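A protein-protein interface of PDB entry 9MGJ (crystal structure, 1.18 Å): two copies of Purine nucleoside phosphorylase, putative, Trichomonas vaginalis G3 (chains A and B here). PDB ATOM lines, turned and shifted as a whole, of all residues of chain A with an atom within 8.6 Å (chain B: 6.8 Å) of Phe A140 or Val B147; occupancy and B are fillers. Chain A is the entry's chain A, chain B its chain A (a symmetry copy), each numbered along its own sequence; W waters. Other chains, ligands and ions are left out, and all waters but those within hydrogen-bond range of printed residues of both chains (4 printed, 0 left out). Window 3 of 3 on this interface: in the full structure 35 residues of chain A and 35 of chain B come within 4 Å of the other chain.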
ATOM      1  N   ILE A 114       6.900 -15.891 -19.365  1.00  0.00           N
ATOM      2  CA  ILE A 114       7.699 -14.944 -18.604  1.00  0.00           C
ATOM      3  C   ILE A 114       6.985 -13.603 -18.660  1.00  0.00           C
ATOM      4  O   ILE A 114       6.699 -13.096 -19.745  1.00  0.00           O
ATOM      5  CB  ILE A 114       9.129 -14.861 -19.166  1.00  0.00           C
ATOM      6  CG1 ILE A 114       9.864 -16.199 -18.958  1.00  0.00           C
ATOM      7  CG2 ILE A 114       9.887 -13.719 -18.501  1.00  0.00           C
ATOM      8  CD1 ILE A 114      11.182 -16.306 -19.754  1.00  0.00           C
ATOM      9  N   VAL A 115       6.717 -13.024 -17.497  1.00  0.00           N
ATOM     10  CA  VAL A 115       5.823 -11.875 -17.380  1.00  0.00           C
ATOM     11  C   VAL A 115       6.609 -10.566 -17.439  1.00  0.00           C
ATOM     12  O   VAL A 115       7.501 -10.324 -16.619  1.00  0.00           O
ATOM     13  CB  VAL A 115       5.035 -11.983 -16.067  1.00  0.00           C
ATOM     14  CG1 VAL A 115       4.163 -10.760 -15.885  1.00  0.00           C
ATOM     15  CG2 VAL A 115       4.199 -13.240 -16.062  1.00  0.00           C
ATOM     16  N   THR A 116       6.226  -9.681 -18.366  1.00  0.00           N
ATOM     17  CA  THR A 116       6.831  -8.359 -18.428  1.00  0.00           C
ATOM     18  C   THR A 116       6.064  -7.327 -17.601  1.00  0.00           C
ATOM     19  O   THR A 116       6.677  -6.430 -17.022  1.00  0.00           O
ATOM     20  CB  THR A 116       6.881  -7.896 -19.879  1.00  0.00           C
ATOM     21  OG1 THR A 116       5.584  -8.081 -20.457  1.00  0.00           O
ATOM     22  CG2 THR A 116       7.951  -8.658 -20.667  1.00  0.00           C
ATOM     23  N   THR A 137       5.048  -3.784 -13.133  1.00  0.00           N
ATOM     24  CA  THR A 137       6.044  -4.002 -14.174  1.00  0.00           C
ATOM     25  C   THR A 137       7.211  -4.797 -13.597  1.00  0.00           C
ATOM     26  O   THR A 137       7.813  -4.399 -12.595  1.00  0.00           O
ATOM     27  CB  THR A 137       6.523  -2.645 -14.735  1.00  0.00           C
ATOM     28  OG1 THR A 137       5.395  -1.855 -15.130  1.00  0.00           O
ATOM     29  CG2 THR A 137       7.403  -2.835 -15.955  1.00  0.00           C
ATOM     30  N   ALA A 138       7.575  -5.876 -14.280  1.00  0.00           N
ATOM     31  CA  ALA A 138       8.720  -6.667 -13.866  1.00  0.00           C
ATOM     32  C   ALA A 138      10.010  -5.909 -14.165  1.00  0.00           C
ATOM     33  O   ALA A 138      10.107  -5.146 -15.136  1.00  0.00           O
ATOM     34  CB  ALA A 138       8.729  -8.003 -14.611  1.00  0.00           C
ATOM     35  N   ASN A 139      11.020  -6.132 -13.332  1.00  0.00           N
ATOM     36  CA  ASN A 139      12.332  -5.559 -13.566  1.00  0.00           C
ATOM     37  C   ASN A 139      12.979  -6.180 -14.803  1.00  0.00           C
ATOM     38  O   ASN A 139      12.938  -7.400 -15.002  1.00  0.00           O
ATOM     39  CB  ASN A 139      13.196  -5.814 -12.330  1.00  0.00           C
ATOM     40  CG  ASN A 139      14.643  -5.471 -12.575  1.00  0.00           C
ATOM     41  OD1 ASN A 139      15.436  -6.323 -12.966  1.00  0.00           O
ATOM     42  ND2 ASN A 139      14.996  -4.226 -12.341  1.00  0.00           N
ATOM     43  N   PHE A 140      13.588  -5.329 -15.643  1.00  0.00           N
ATOM     44  CA  PHE A 140      14.111  -5.812 -16.915  1.00  0.00           C
ATOM     45  C   PHE A 140      15.248  -6.818 -16.744  1.00  0.00           C
ATOM     46  O   PHE A 140      15.334  -7.778 -17.508  1.00  0.00           O
ATOM     47  CB  PHE A 140      14.536  -4.632 -17.794  1.00  0.00           C
ATOM     48  CG  PHE A 140      15.195  -5.070 -19.065  1.00  0.00           C
ATOM     49  CD1 PHE A 140      14.433  -5.526 -20.133  1.00  0.00           C
ATOM     50  CD2 PHE A 140      16.583  -5.112 -19.169  1.00  0.00           C
ATOM     51  CE1 PHE A 140      15.038  -5.969 -21.301  1.00  0.00           C
ATOM     52  CE2 PHE A 140      17.200  -5.559 -20.342  1.00  0.00           C
ATOM     53  CZ  PHE A 140      16.419  -6.003 -21.397  1.00  0.00           C
ATOM     54  N   GLU A 141      16.148  -6.589 -15.791  1.00  0.00           N
ATOM     55  CA  GLU A 141      17.226  -7.544 -15.570  1.00  0.00           C
ATOM     56  C   GLU A 141      16.664  -8.903 -15.186  1.00  0.00           C
ATOM     57  O   GLU A 141      17.199  -9.937 -15.605  1.00  0.00           O
ATOM     58  CB  GLU A 141      18.196  -7.016 -14.512  1.00  0.00           C
ATOM     59  CG  GLU A 141      19.179  -5.948 -14.990  1.00  0.00           C
ATOM     60  CD  GLU A 141      18.560  -4.607 -15.257  1.00  0.00           C
ATOM     61  OE1 GLU A 141      17.562  -4.251 -14.599  1.00  0.00           O
ATOM     62  OE2 GLU A 141      19.101  -3.892 -16.123  1.00  0.00           O
ATOM     63  N   VAL A 142      15.586  -8.935 -14.393  1.00  0.00           N
ATOM     64  CA  VAL A 142      14.979 -10.215 -14.028  1.00  0.00           C
ATOM     65  C   VAL A 142      14.353 -10.885 -15.246  1.00  0.00           C
ATOM     66  O   VAL A 142      14.547 -12.084 -15.481  1.00  0.00           O
ATOM     67  CB  VAL A 142      13.948 -10.035 -12.900  1.00  0.00           C
ATOM     68  CG1 VAL A 142      13.260 -11.361 -12.583  1.00  0.00           C
ATOM     69  CG2 VAL A 142      14.612  -9.495 -11.657  1.00  0.00           C
ATOM     70  N   VAL A 143      13.569 -10.128 -16.025  1.00  0.00           N
ATOM     71  CA  VAL A 143      12.963 -10.699 -17.223  1.00  0.00           C
ATOM     72  C   VAL A 143      14.048 -11.272 -18.122  1.00  0.00           C
ATOM     73  O   VAL A 143      13.951 -12.397 -18.618  1.00  0.00           O
ATOM     74  CB  VAL A 143      12.137  -9.630 -17.966  1.00  0.00           C
ATOM     75  CG1 VAL A 143      11.592 -10.210 -19.257  1.00  0.00           C
ATOM     76  CG2 VAL A 143      11.007  -9.115 -17.097  1.00  0.00           C
ATOM     77  N   SER A 144      15.092 -10.479 -18.350  1.00  0.00           N
ATOM     78  CA  SER A 144      16.168 -10.906 -19.238  1.00  0.00           C
ATOM     79  C   SER A 144      16.866 -12.146 -18.708  1.00  0.00           C
ATOM     80  O   SER A 144      17.219 -13.042 -19.481  1.00  0.00           O
ATOM     81  CB  SER A 144      17.183  -9.777 -19.411  1.00  0.00           C
ATOM     82  OG  SER A 144      18.253 -10.187 -20.262  1.00  0.00           O
ATOM     83  N   ALA A 145      17.084 -12.215 -17.399  1.00  0.00           N
ATOM     84  CA  ALA A 145      17.736 -13.398 -16.856  1.00  0.00           C
ATOM     85  C   ALA A 145      16.886 -14.637 -17.096  1.00  0.00           C
ATOM     86  O   ALA A 145      17.422 -15.714 -17.396  1.00  0.00           O
ATOM     87  CB  ALA A 145      18.043 -13.217 -15.372  1.00  0.00           C
ATOM     88  N   LEU A 146      15.567 -14.524 -16.934  1.00  0.00           N
ATOM     89  CA  LEU A 146      14.682 -15.656 -17.199  1.00  0.00           C
ATOM     90  C   LEU A 146      14.718 -16.036 -18.676  1.00  0.00           C
ATOM     91  O   LEU A 146      14.830 -17.221 -19.023  1.00  0.00           O
ATOM     92  CB  LEU A 146      13.263 -15.329 -16.728  1.00  0.00           C
ATOM     93  CG  LEU A 146      13.126 -15.172 -15.214  1.00  0.00           C
ATOM     94  CD1 LEU A 146      11.797 -14.461 -14.883  1.00  0.00           C
ATOM     95  CD2 LEU A 146      13.116 -16.510 -14.527  1.00  0.00           C
ATOM     96  N   VAL A 147      14.649 -15.042 -19.566  1.00  0.00           N
ATOM     97  CA  VAL A 147      14.665 -15.320 -21.003  1.00  0.00           C
ATOM     98  C   VAL A 147      15.962 -16.009 -21.403  1.00  0.00           C
ATOM     99  O   VAL A 147      15.960 -16.993 -22.146  1.00  0.00           O
ATOM    100  CB  VAL A 147      14.437 -14.022 -21.795  1.00  0.00           C
ATOM    101  CG1 VAL A 147      14.731 -14.242 -23.269  1.00  0.00           C
ATOM    102  CG2 VAL A 147      13.016 -13.537 -21.626  1.00  0.00           C
ATOM    103  N   GLU A 148      17.091 -15.485 -20.933  1.00  0.00           N
ATOM    104  CA  GLU A 148      18.383 -16.025 -21.328  1.00  0.00           C
ATOM    105  C   GLU A 148      18.598 -17.407 -20.742  1.00  0.00           C
ATOM    106  O   GLU A 148      19.199 -18.270 -21.390  1.00  0.00           O
ATOM    107  CB  GLU A 148      19.486 -15.070 -20.882  1.00  0.00           C
ATOM    108  CG  GLU A 148      19.527 -13.777 -21.677  1.00  0.00           C
ATOM    109  CD  GLU A 148      19.553 -14.017 -23.187  1.00  0.00           C
ATOM    110  OE1 GLU A 148      20.441 -14.763 -23.660  1.00  0.00           O
ATOM    111  OE2 GLU A 148      18.666 -13.491 -23.893  1.00  0.00           O
ATOM    112  N   VAL A 159       6.670 -14.499 -23.835  1.00  0.00           N
ATOM    113  CA  VAL A 159       7.054 -13.348 -23.027  1.00  0.00           C
ATOM    114  C   VAL A 159       6.000 -12.271 -23.229  1.00  0.00           C
ATOM    115  O   VAL A 159       5.728 -11.878 -24.361  1.00  0.00           O
ATOM    116  CB  VAL A 159       8.446 -12.828 -23.430  1.00  0.00           C
ATOM    117  CG1 VAL A 159       8.866 -11.670 -22.542  1.00  0.00           C
ATOM    118  CG2 VAL A 159       9.480 -13.958 -23.382  1.00  0.00           C
ATOM    119  N   ALA A 203      13.797  -2.307  -5.192  1.00  0.00           N
ATOM    120  CA  ALA A 203      14.218  -3.689  -5.363  1.00  0.00           C
ATOM    121  C   ALA A 203      13.644  -4.223  -6.675  1.00  0.00           C
ATOM    122  O   ALA A 203      13.063  -3.477  -7.476  1.00  0.00           O
ATOM    123  CB  ALA A 203      13.785  -4.522  -4.148  1.00  0.00           C
ATOM    124  N   ARG A 204      13.809  -5.524  -6.891  1.00  0.00           N
ATOM    125  CA  ARG A 204      13.502  -6.135  -8.170  1.00  0.00           C
ATOM    126  C   ARG A 204      12.587  -7.330  -7.995  1.00  0.00           C
ATOM    127  O   ARG A 204      12.671  -8.068  -7.009  1.00  0.00           O
ATOM    128  CB  ARG A 204      14.787  -6.607  -8.858  1.00  0.00           C
ATOM    129  CG  ARG A 204      15.767  -5.503  -9.080  1.00  0.00           C
ATOM    130  CD  ARG A 204      16.924  -6.008  -9.868  1.00  0.00           C
ATOM    131  NE  ARG A 204      17.576  -7.128  -9.206  1.00  0.00           N
ATOM    132  CZ  ARG A 204      18.721  -7.648  -9.599  1.00  0.00           C
ATOM    133  NH1 ARG A 204      19.384  -7.148 -10.627  1.00  0.00           N
ATOM    134  NH2 ARG A 204      19.216  -8.691  -8.939  1.00  0.00           N
ATOM    135  N   ALA A 205      11.750  -7.542  -9.006  1.00  0.00           N
ATOM    136  CA  ALA A 205      10.854  -8.679  -9.033  1.00  0.00           C
ATOM    137  C   ALA A 205      10.595  -9.114 -10.466  1.00  0.00           C
ATOM    138  O   ALA A 205      10.709  -8.327 -11.417  1.00  0.00           O
ATOM    139  CB  ALA A 205       9.542  -8.405  -8.297  1.00  0.00           C
ATOM    140  N   GLY A 206      10.201 -10.373 -10.604  1.00  0.00           N
ATOM    141  CA  GLY A 206       9.714 -10.913 -11.849  1.00  0.00           C
ATOM    142  C   GLY A 206       8.791 -12.078 -11.580  1.00  0.00           C
ATOM    143  O   GLY A 206       8.524 -12.439 -10.426  1.00  0.00           O
ATOM    144  N   LEU A 244      21.520 -12.872 -11.016  1.00  0.00           N
ATOM    145  CA  LEU A 244      20.827 -11.804 -10.286  1.00  0.00           C
ATOM    146  C   LEU A 244      21.306 -11.587  -8.843  1.00  0.00           C
ATOM    147  O   LEU A 244      20.832 -10.632  -8.204  1.00  0.00           O
ATOM    148  CB  LEU A 244      19.330 -12.119 -10.253  1.00  0.00           C
ATOM    149  CG  LEU A 244      18.630 -12.117 -11.614  1.00  0.00           C
ATOM    150  CD1 LEU A 244      17.272 -12.757 -11.457  1.00  0.00           C
ATOM    151  CD2 LEU A 244      18.516 -10.721 -12.222  1.00  0.00           C
ATOM    152  OXT LEU A 244      22.118 -12.331  -8.278  1.00  0.00           O
ATOM    153  N   ILE B 114      14.853   3.838 -21.547  1.00  0.00           N
ATOM    154  CA  ILE B 114      14.166   2.841 -22.353  1.00  0.00           C
ATOM    155  C   ILE B 114      12.975   2.352 -21.544  1.00  0.00           C
ATOM    156  O   ILE B 114      13.137   1.900 -20.410  1.00  0.00           O
ATOM    157  CB  ILE B 114      15.118   1.693 -22.732  1.00  0.00           C
ATOM    158  CG1 ILE B 114      16.228   2.207 -23.668  1.00  0.00           C
ATOM    159  CG2 ILE B 114      14.338   0.561 -23.388  1.00  0.00           C
ATOM    160  CD1 ILE B 114      17.389   1.206 -23.851  1.00  0.00           C
ATOM    161  N   THR B 116       9.857   0.162 -20.307  1.00  0.00           N
ATOM    162  CA  THR B 116       9.309  -1.186 -20.267  1.00  0.00           C
ATOM    163  C   THR B 116       7.783  -1.193 -20.188  1.00  0.00           C
ATOM    164  O   THR B 116       7.146  -2.079 -20.758  1.00  0.00           O
ATOM    165  CB  THR B 116       9.874  -1.924 -19.058  1.00  0.00           C
ATOM    166  OG1 THR B 116       9.716  -1.089 -17.906  1.00  0.00           O
ATOM    167  CG2 THR B 116      11.344  -2.297 -19.274  1.00  0.00           C
ATOM    168  N   PHE B 140       8.900  -7.052 -25.560  1.00  0.00           N
ATOM    169  CA  PHE B 140      10.209  -7.387 -25.011  1.00  0.00           C
ATOM    170  C   PHE B 140      11.313  -7.383 -26.068  1.00  0.00           C
ATOM    171  O   PHE B 140      12.431  -6.961 -25.779  1.00  0.00           O
ATOM    172  CB  PHE B 140      10.146  -8.729 -24.275  1.00  0.00           C
ATOM    173  CG  PHE B 140      11.488  -9.186 -23.795  1.00  0.00           C
ATOM    174  CD1 PHE B 140      12.049  -8.640 -22.648  1.00  0.00           C
ATOM    175  CD2 PHE B 140      12.235 -10.098 -24.534  1.00  0.00           C
ATOM    176  CE1 PHE B 140      13.309  -9.030 -22.216  1.00  0.00           C
ATOM    177  CE2 PHE B 140      13.507 -10.495 -24.108  1.00  0.00           C
ATOM    178  CZ  PHE B 140      14.043  -9.941 -22.956  1.00  0.00           C
ATOM    179  N   VAL B 142      11.498  -5.501 -28.626  1.00  0.00           N
ATOM    180  CA  VAL B 142      11.841  -4.102 -28.886  1.00  0.00           C
ATOM    181  C   VAL B 142      12.695  -3.534 -27.758  1.00  0.00           C
ATOM    182  O   VAL B 142      13.715  -2.877 -28.003  1.00  0.00           O
ATOM    183  CB  VAL B 142      10.576  -3.256 -29.106  1.00  0.00           C
ATOM    184  CG1 VAL B 142      10.938  -1.784 -29.295  1.00  0.00           C
ATOM    185  CG2 VAL B 142       9.810  -3.751 -30.310  1.00  0.00           C
ATOM    186  N   VAL B 143      12.277  -3.754 -26.504  1.00  0.00           N
ATOM    187  CA  VAL B 143      13.064  -3.264 -25.378  1.00  0.00           C
ATOM    188  C   VAL B 143      14.481  -3.809 -25.467  1.00  0.00           C
ATOM    189  O   VAL B 143      15.466  -3.080 -25.322  1.00  0.00           O
ATOM    190  CB  VAL B 143      12.399  -3.667 -24.046  1.00  0.00           C
ATOM    191  CG1 VAL B 143      13.275  -3.235 -22.886  1.00  0.00           C
ATOM    192  CG2 VAL B 143      11.016  -3.059 -23.922  1.00  0.00           C
ATOM    193  N   SER B 144      14.588  -5.116 -25.693  1.00  0.00           N
ATOM    194  CA  SER B 144      15.898  -5.755 -25.748  1.00  0.00           C
ATOM    195  C   SER B 144      16.738  -5.203 -26.886  1.00  0.00           C
ATOM    196  O   SER B 144      17.947  -5.005 -26.730  1.00  0.00           O
ATOM    197  CB  SER B 144      15.737  -7.266 -25.912  1.00  0.00           C
ATOM    198  OG  SER B 144      17.012  -7.903 -25.988  1.00  0.00           O
ATOM    199  N   ALA B 145      16.124  -4.957 -28.039  1.00  0.00           N
ATOM    200  CA  ALA B 145      16.897  -4.410 -29.144  1.00  0.00           C
ATOM    201  C   ALA B 145      17.450  -3.039 -28.788  1.00  0.00           C
ATOM    202  O   ALA B 145      18.589  -2.710 -29.149  1.00  0.00           O
ATOM    203  CB  ALA B 145      16.059  -4.354 -30.419  1.00  0.00           C
ATOM    204  N   LEU B 146      16.654  -2.206 -28.114  1.00  0.00           N
ATOM    205  CA  LEU B 146      17.135  -0.894 -27.689  1.00  0.00           C
ATOM    206  C   LEU B 146      18.263  -1.034 -26.672  1.00  0.00           C
ATOM    207  O   LEU B 146      19.299  -0.362 -26.779  1.00  0.00           O
ATOM    208  CB  LEU B 146      15.970  -0.067 -27.139  1.00  0.00           C
ATOM    209  CG  LEU B 146      14.919   0.308 -28.184  1.00  0.00           C
ATOM    210  CD1 LEU B 146      13.627   0.768 -27.479  1.00  0.00           C
ATOM    211  CD2 LEU B 146      15.396   1.437 -29.055  1.00  0.00           C
ATOM    212  N   VAL B 147      18.094  -1.922 -25.687  1.00  0.00           N
ATOM    213  CA  VAL B 147      19.122  -2.111 -24.663  1.00  0.00           C
ATOM    214  C   VAL B 147      20.426  -2.583 -25.290  1.00  0.00           C
ATOM    215  O   VAL B 147      21.507  -2.081 -24.973  1.00  0.00           O
ATOM    216  CB  VAL B 147      18.619  -3.081 -23.582  1.00  0.00           C
ATOM    217  CG1 VAL B 147      19.764  -3.504 -22.676  1.00  0.00           C
ATOM    218  CG2 VAL B 147      17.526  -2.443 -22.759  1.00  0.00           C
ATOM    219  N   GLU B 148      20.343  -3.575 -26.174  1.00  0.00           N
ATOM    220  CA  GLU B 148      21.543  -4.149 -26.764  1.00  0.00           C
ATOM    221  C   GLU B 148      22.215  -3.162 -27.699  1.00  0.00           C
ATOM    222  O   GLU B 148      23.447  -3.119 -27.775  1.00  0.00           O
ATOM    223  CB  GLU B 148      21.178  -5.432 -27.501  1.00  0.00           C
ATOM    224  CG  GLU B 148      20.808  -6.579 -26.576  1.00  0.00           C
ATOM    225  CD  GLU B 148      21.859  -6.820 -25.491  1.00  0.00           C
ATOM    226  OE1 GLU B 148      23.048  -7.003 -25.838  1.00  0.00           O
ATOM    227  OE2 GLU B 148      21.502  -6.791 -24.294  1.00  0.00           O
ATOM    228  N   SER B 149      21.425  -2.375 -28.426  1.00  0.00           N
ATOM    229  CA  SER B 149      22.014  -1.365 -29.294  1.00  0.00           C
ATOM    230  C   SER B 149      22.783  -0.327 -28.488  1.00  0.00           C
ATOM    231  O   SER B 149      23.897   0.059 -28.867  1.00  0.00           O
ATOM    232  CB  SER B 149      20.941  -0.705 -30.153  1.00  0.00           C
ATOM    233  OG  SER B 149      20.379  -1.633 -31.068  1.00  0.00           O
ATOM    234  N   ALA B 150      22.214   0.132 -27.370  1.00  0.00           N
ATOM    235  CA  ALA B 150      22.914   1.108 -26.543  1.00  0.00           C
ATOM    236  C   ALA B 150      24.194   0.520 -25.974  1.00  0.00           C
ATOM    237  O   ALA B 150      25.228   1.194 -25.922  1.00  0.00           O
ATOM    238  CB  ALA B 150      21.997   1.603 -25.429  1.00  0.00           C
ATOM    239  N   LYS B 151      24.151  -0.745 -25.559  1.00  0.00           N
ATOM    240  CA  LYS B 151      25.356  -1.397 -25.057  1.00  0.00           C
ATOM    241  C   LYS B 151      26.446  -1.430 -26.119  1.00  0.00           C
ATOM    242  O   LYS B 151      27.612  -1.136 -25.835  1.00  0.00           O
ATOM    243  CB  LYS B 151      25.035  -2.819 -24.613  1.00  0.00           C
ATOM    244  CG  LYS B 151      24.378  -2.911 -23.265  1.00  0.00           C
ATOM    245  CD  LYS B 151      24.037  -4.347 -22.952  1.00  0.00           C
ATOM    246  CE  LYS B 151      23.265  -4.486 -21.654  1.00  0.00           C
ATOM    247  NZ  LYS B 151      22.888  -5.910 -21.389  1.00  0.00           N
ATOM    248  N   ALA B 152      26.087  -1.794 -27.350  1.00  0.00           N
ATOM    249  CA  ALA B 152      27.083  -1.860 -28.412  1.00  0.00           C
ATOM    250  C   ALA B 152      27.671  -0.488 -28.714  1.00  0.00           C
ATOM    251  O   ALA B 152      28.841  -0.389 -29.100  1.00  0.00           O
ATOM    252  CB  ALA B 152      26.466  -2.474 -29.668  1.00  0.00           C
ATOM    253  N   ILE B 155      26.594   3.537 -24.763  1.00  0.00           N
ATOM    254  CA  ILE B 155      25.756   4.621 -24.256  1.00  0.00           C
ATOM    255  C   ILE B 155      24.981   4.088 -23.055  1.00  0.00           C
ATOM    256  O   ILE B 155      24.181   3.160 -23.218  1.00  0.00           O
ATOM    257  CB  ILE B 155      24.798   5.154 -25.337  1.00  0.00           C
ATOM    258  CG1 ILE B 155      25.571   5.715 -26.534  1.00  0.00           C
ATOM    259  CG2 ILE B 155      23.879   6.219 -24.741  1.00  0.00           C
ATOM    260  CD1 ILE B 155      24.708   5.968 -27.744  1.00  0.00           C
ATOM    261  N   THR B 157      22.111   3.577 -20.254  1.00  0.00           N
ATOM    262  CA  THR B 157      20.667   3.745 -20.288  1.00  0.00           C
ATOM    263  C   THR B 157      20.046   3.436 -18.933  1.00  0.00           C
ATOM    264  O   THR B 157      20.556   2.622 -18.158  1.00  0.00           O
ATOM    265  CB  THR B 157      20.007   2.809 -21.311  1.00  0.00           C
ATOM    266  OG1 THR B 157      20.278   1.445 -20.943  1.00  0.00           O
ATOM    267  CG2 THR B 157      20.544   3.078 -22.717  1.00  0.00           C
ATOM    268  N   GLN B 158      18.907   4.068 -18.694  1.00  0.00           N
ATOM    269  CA  GLN B 158      17.983   3.726 -17.625  1.00  0.00           C
ATOM    270  C   GLN B 158      16.851   2.924 -18.253  1.00  0.00           C
ATOM    271  O   GLN B 158      16.362   3.277 -19.318  1.00  0.00           O
ATOM    272  CB  GLN B 158      17.401   5.002 -17.014  1.00  0.00           C
ATOM    273  CG  GLN B 158      18.433   6.029 -16.577  1.00  0.00           C
ATOM    274  CD  GLN B 158      19.018   5.733 -15.211  1.00  0.00           C
ATOM    275  OE1 GLN B 158      18.667   4.741 -14.575  1.00  0.00           O
ATOM    276  NE2 GLN B 158      19.893   6.616 -14.738  1.00  0.00           N
ATOM    277  N   VAL B 159      16.432   1.843 -17.609  1.00  0.00           N
ATOM    278  CA  VAL B 159      15.385   0.989 -18.156  1.00  0.00           C
ATOM    279  C   VAL B 159      14.291   0.871 -17.105  1.00  0.00           C
ATOM    280  O   VAL B 159      14.563   0.479 -15.974  1.00  0.00           O
ATOM    281  CB  VAL B 159      15.938  -0.401 -18.522  1.00  0.00           C
ATOM    282  CG1 VAL B 159      14.857  -1.263 -19.148  1.00  0.00           C
ATOM    283  CG2 VAL B 159      17.146  -0.273 -19.455  1.00  0.00           C
ATOM    284  N   GLY B 160      13.055   1.218 -17.458  1.00  0.00           N
ATOM    285  CA  GLY B 160      11.987   1.144 -16.469  1.00  0.00           C
ATOM    286  C   GLY B 160      10.724   1.864 -16.922  1.00  0.00           C
ATOM    287  O   GLY B 160      10.490   2.057 -18.118  1.00  0.00           O
ATOM    288  N   ILE B 236      20.722   4.884 -31.147  1.00  0.00           N
ATOM    289  CA  ILE B 236      20.263   3.667 -30.483  1.00  0.00           C
ATOM    290  C   ILE B 236      19.016   3.136 -31.174  1.00  0.00           C
ATOM    291  O   ILE B 236      18.905   1.935 -31.457  1.00  0.00           O
ATOM    292  CB  ILE B 236      19.988   3.942 -28.992  1.00  0.00           C
ATOM    293  CG1 ILE B 236      21.276   4.274 -28.236  1.00  0.00           C
ATOM    294  CG2 ILE B 236      19.266   2.744 -28.349  1.00  0.00           C
ATOM    295  CD1 ILE B 236      21.040   4.886 -26.862  1.00  0.00           C
ATOM    296  N   ALA B 240      18.655  -0.276 -33.349  1.00  0.00           N
ATOM    297  CA  ALA B 240      17.697  -1.268 -32.878  1.00  0.00           C
ATOM    298  C   ALA B 240      16.784  -1.741 -34.000  1.00  0.00           C
ATOM    299  O   ALA B 240      16.419  -2.927 -34.034  1.00  0.00           O
ATOM    300  CB  ALA B 240      16.886  -0.718 -31.709  1.00  0.00           C
HETATM  301  O   HOH W   1       6.880  -9.023 -25.270  1.00  0.00           O
HETATM  302  O   HOH W   2      13.758  -2.531 -15.202  1.00  0.00           O
HETATM  303  O   HOH W   3      16.640  -1.892 -14.585  1.00  0.00           O
HETATM  304  O   HOH W   4      11.028  -2.545 -15.883  1.00  0.00           O
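The backbone carbonyl oxygen (O) of Gly B160 sits at hydrogen-bond distance from the backbone NH (N) of Thr B116 (3.0 Å).
Among the printed residues, merely in contact across the chains: Thr A137 with Thr B116 (3.5 Å), Phe A140 with Phe B140 (3.6 Å), Phe A140 with Val B143 (3.6 Å), Phe A140 with Val B147 (3.96 Å), Phe A140 with Val B159 (3.6 Å), Val A143 with Phe B140 (3.6 Å), Val A147 with Phe B140 (3.96 Å) and Val A159 with Phe B140 (3.6 Å).
Of the printed residues of chain B, Thr A137 touches Thr B116 (3.5 Å). Printed residues of chain B within 4 Å of Phe A140: Phe B140, Val B143, Val B147 and Val B159. Of the printed residues of chain B, Val A159 touches Phe B140. Printed residues of chain A within 4 Å of Phe B140: Phe A140 (3.6 Å), Val A143 (3.6 Å), Val A147 (3.96 Å) and Val A159 (3.6 Å). Val B147 touches just one residue of chain A: Phe A140 (3.96 Å). Lys B151 touches none of the printed residues of chain A. The nearest printed residue of chain B that does not touch Phe A140 is Thr B116 (4.2 Å).
Printed residues of chain B that touch a printed residue of chain A: Thr B116, Phe B140, Val B143, Val B147 and Val B159. Hydrophobic or aromatic side chains of chain A that line the printed part of chain B: Phe A140, Val A143, Val A147 and Val A159. Among the printed residues, no Asp or Glu carboxylate lies within 4 Å of a Lys or Arg side-chain nitrogen of the other chain.
Phe B140 touches its own counterpart, Phe A140. Phe A140 touches Val B143, and with the chains exchanged Val A143 touches Phe B140. Phe A140 touches Val B147, and with the chains exchanged Val A147 touches Phe B140. Phe A140 touches Val B159, and with the chains exchanged Val A159 touches Phe B140. Positions printed for both chains: 114, 116, 140, 142, 143, 144, 145, 146, 147, 148 and 159.
Water W3 bridges OE1 of Glu A141 (2.5 Å) and O of Val B159 (3.4 Å). Water W4 lies within hydrogen-bond range of OG1 of Thr B116 (2.8 Å) and O of Ala A138 (2.9 Å). Water W1 bridges N of Phe B140 and O of Val A159. Water W2 bridges the backbone NH (N) of Phe A140 and the backbone carbonyl oxygen (O) of Val B159.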
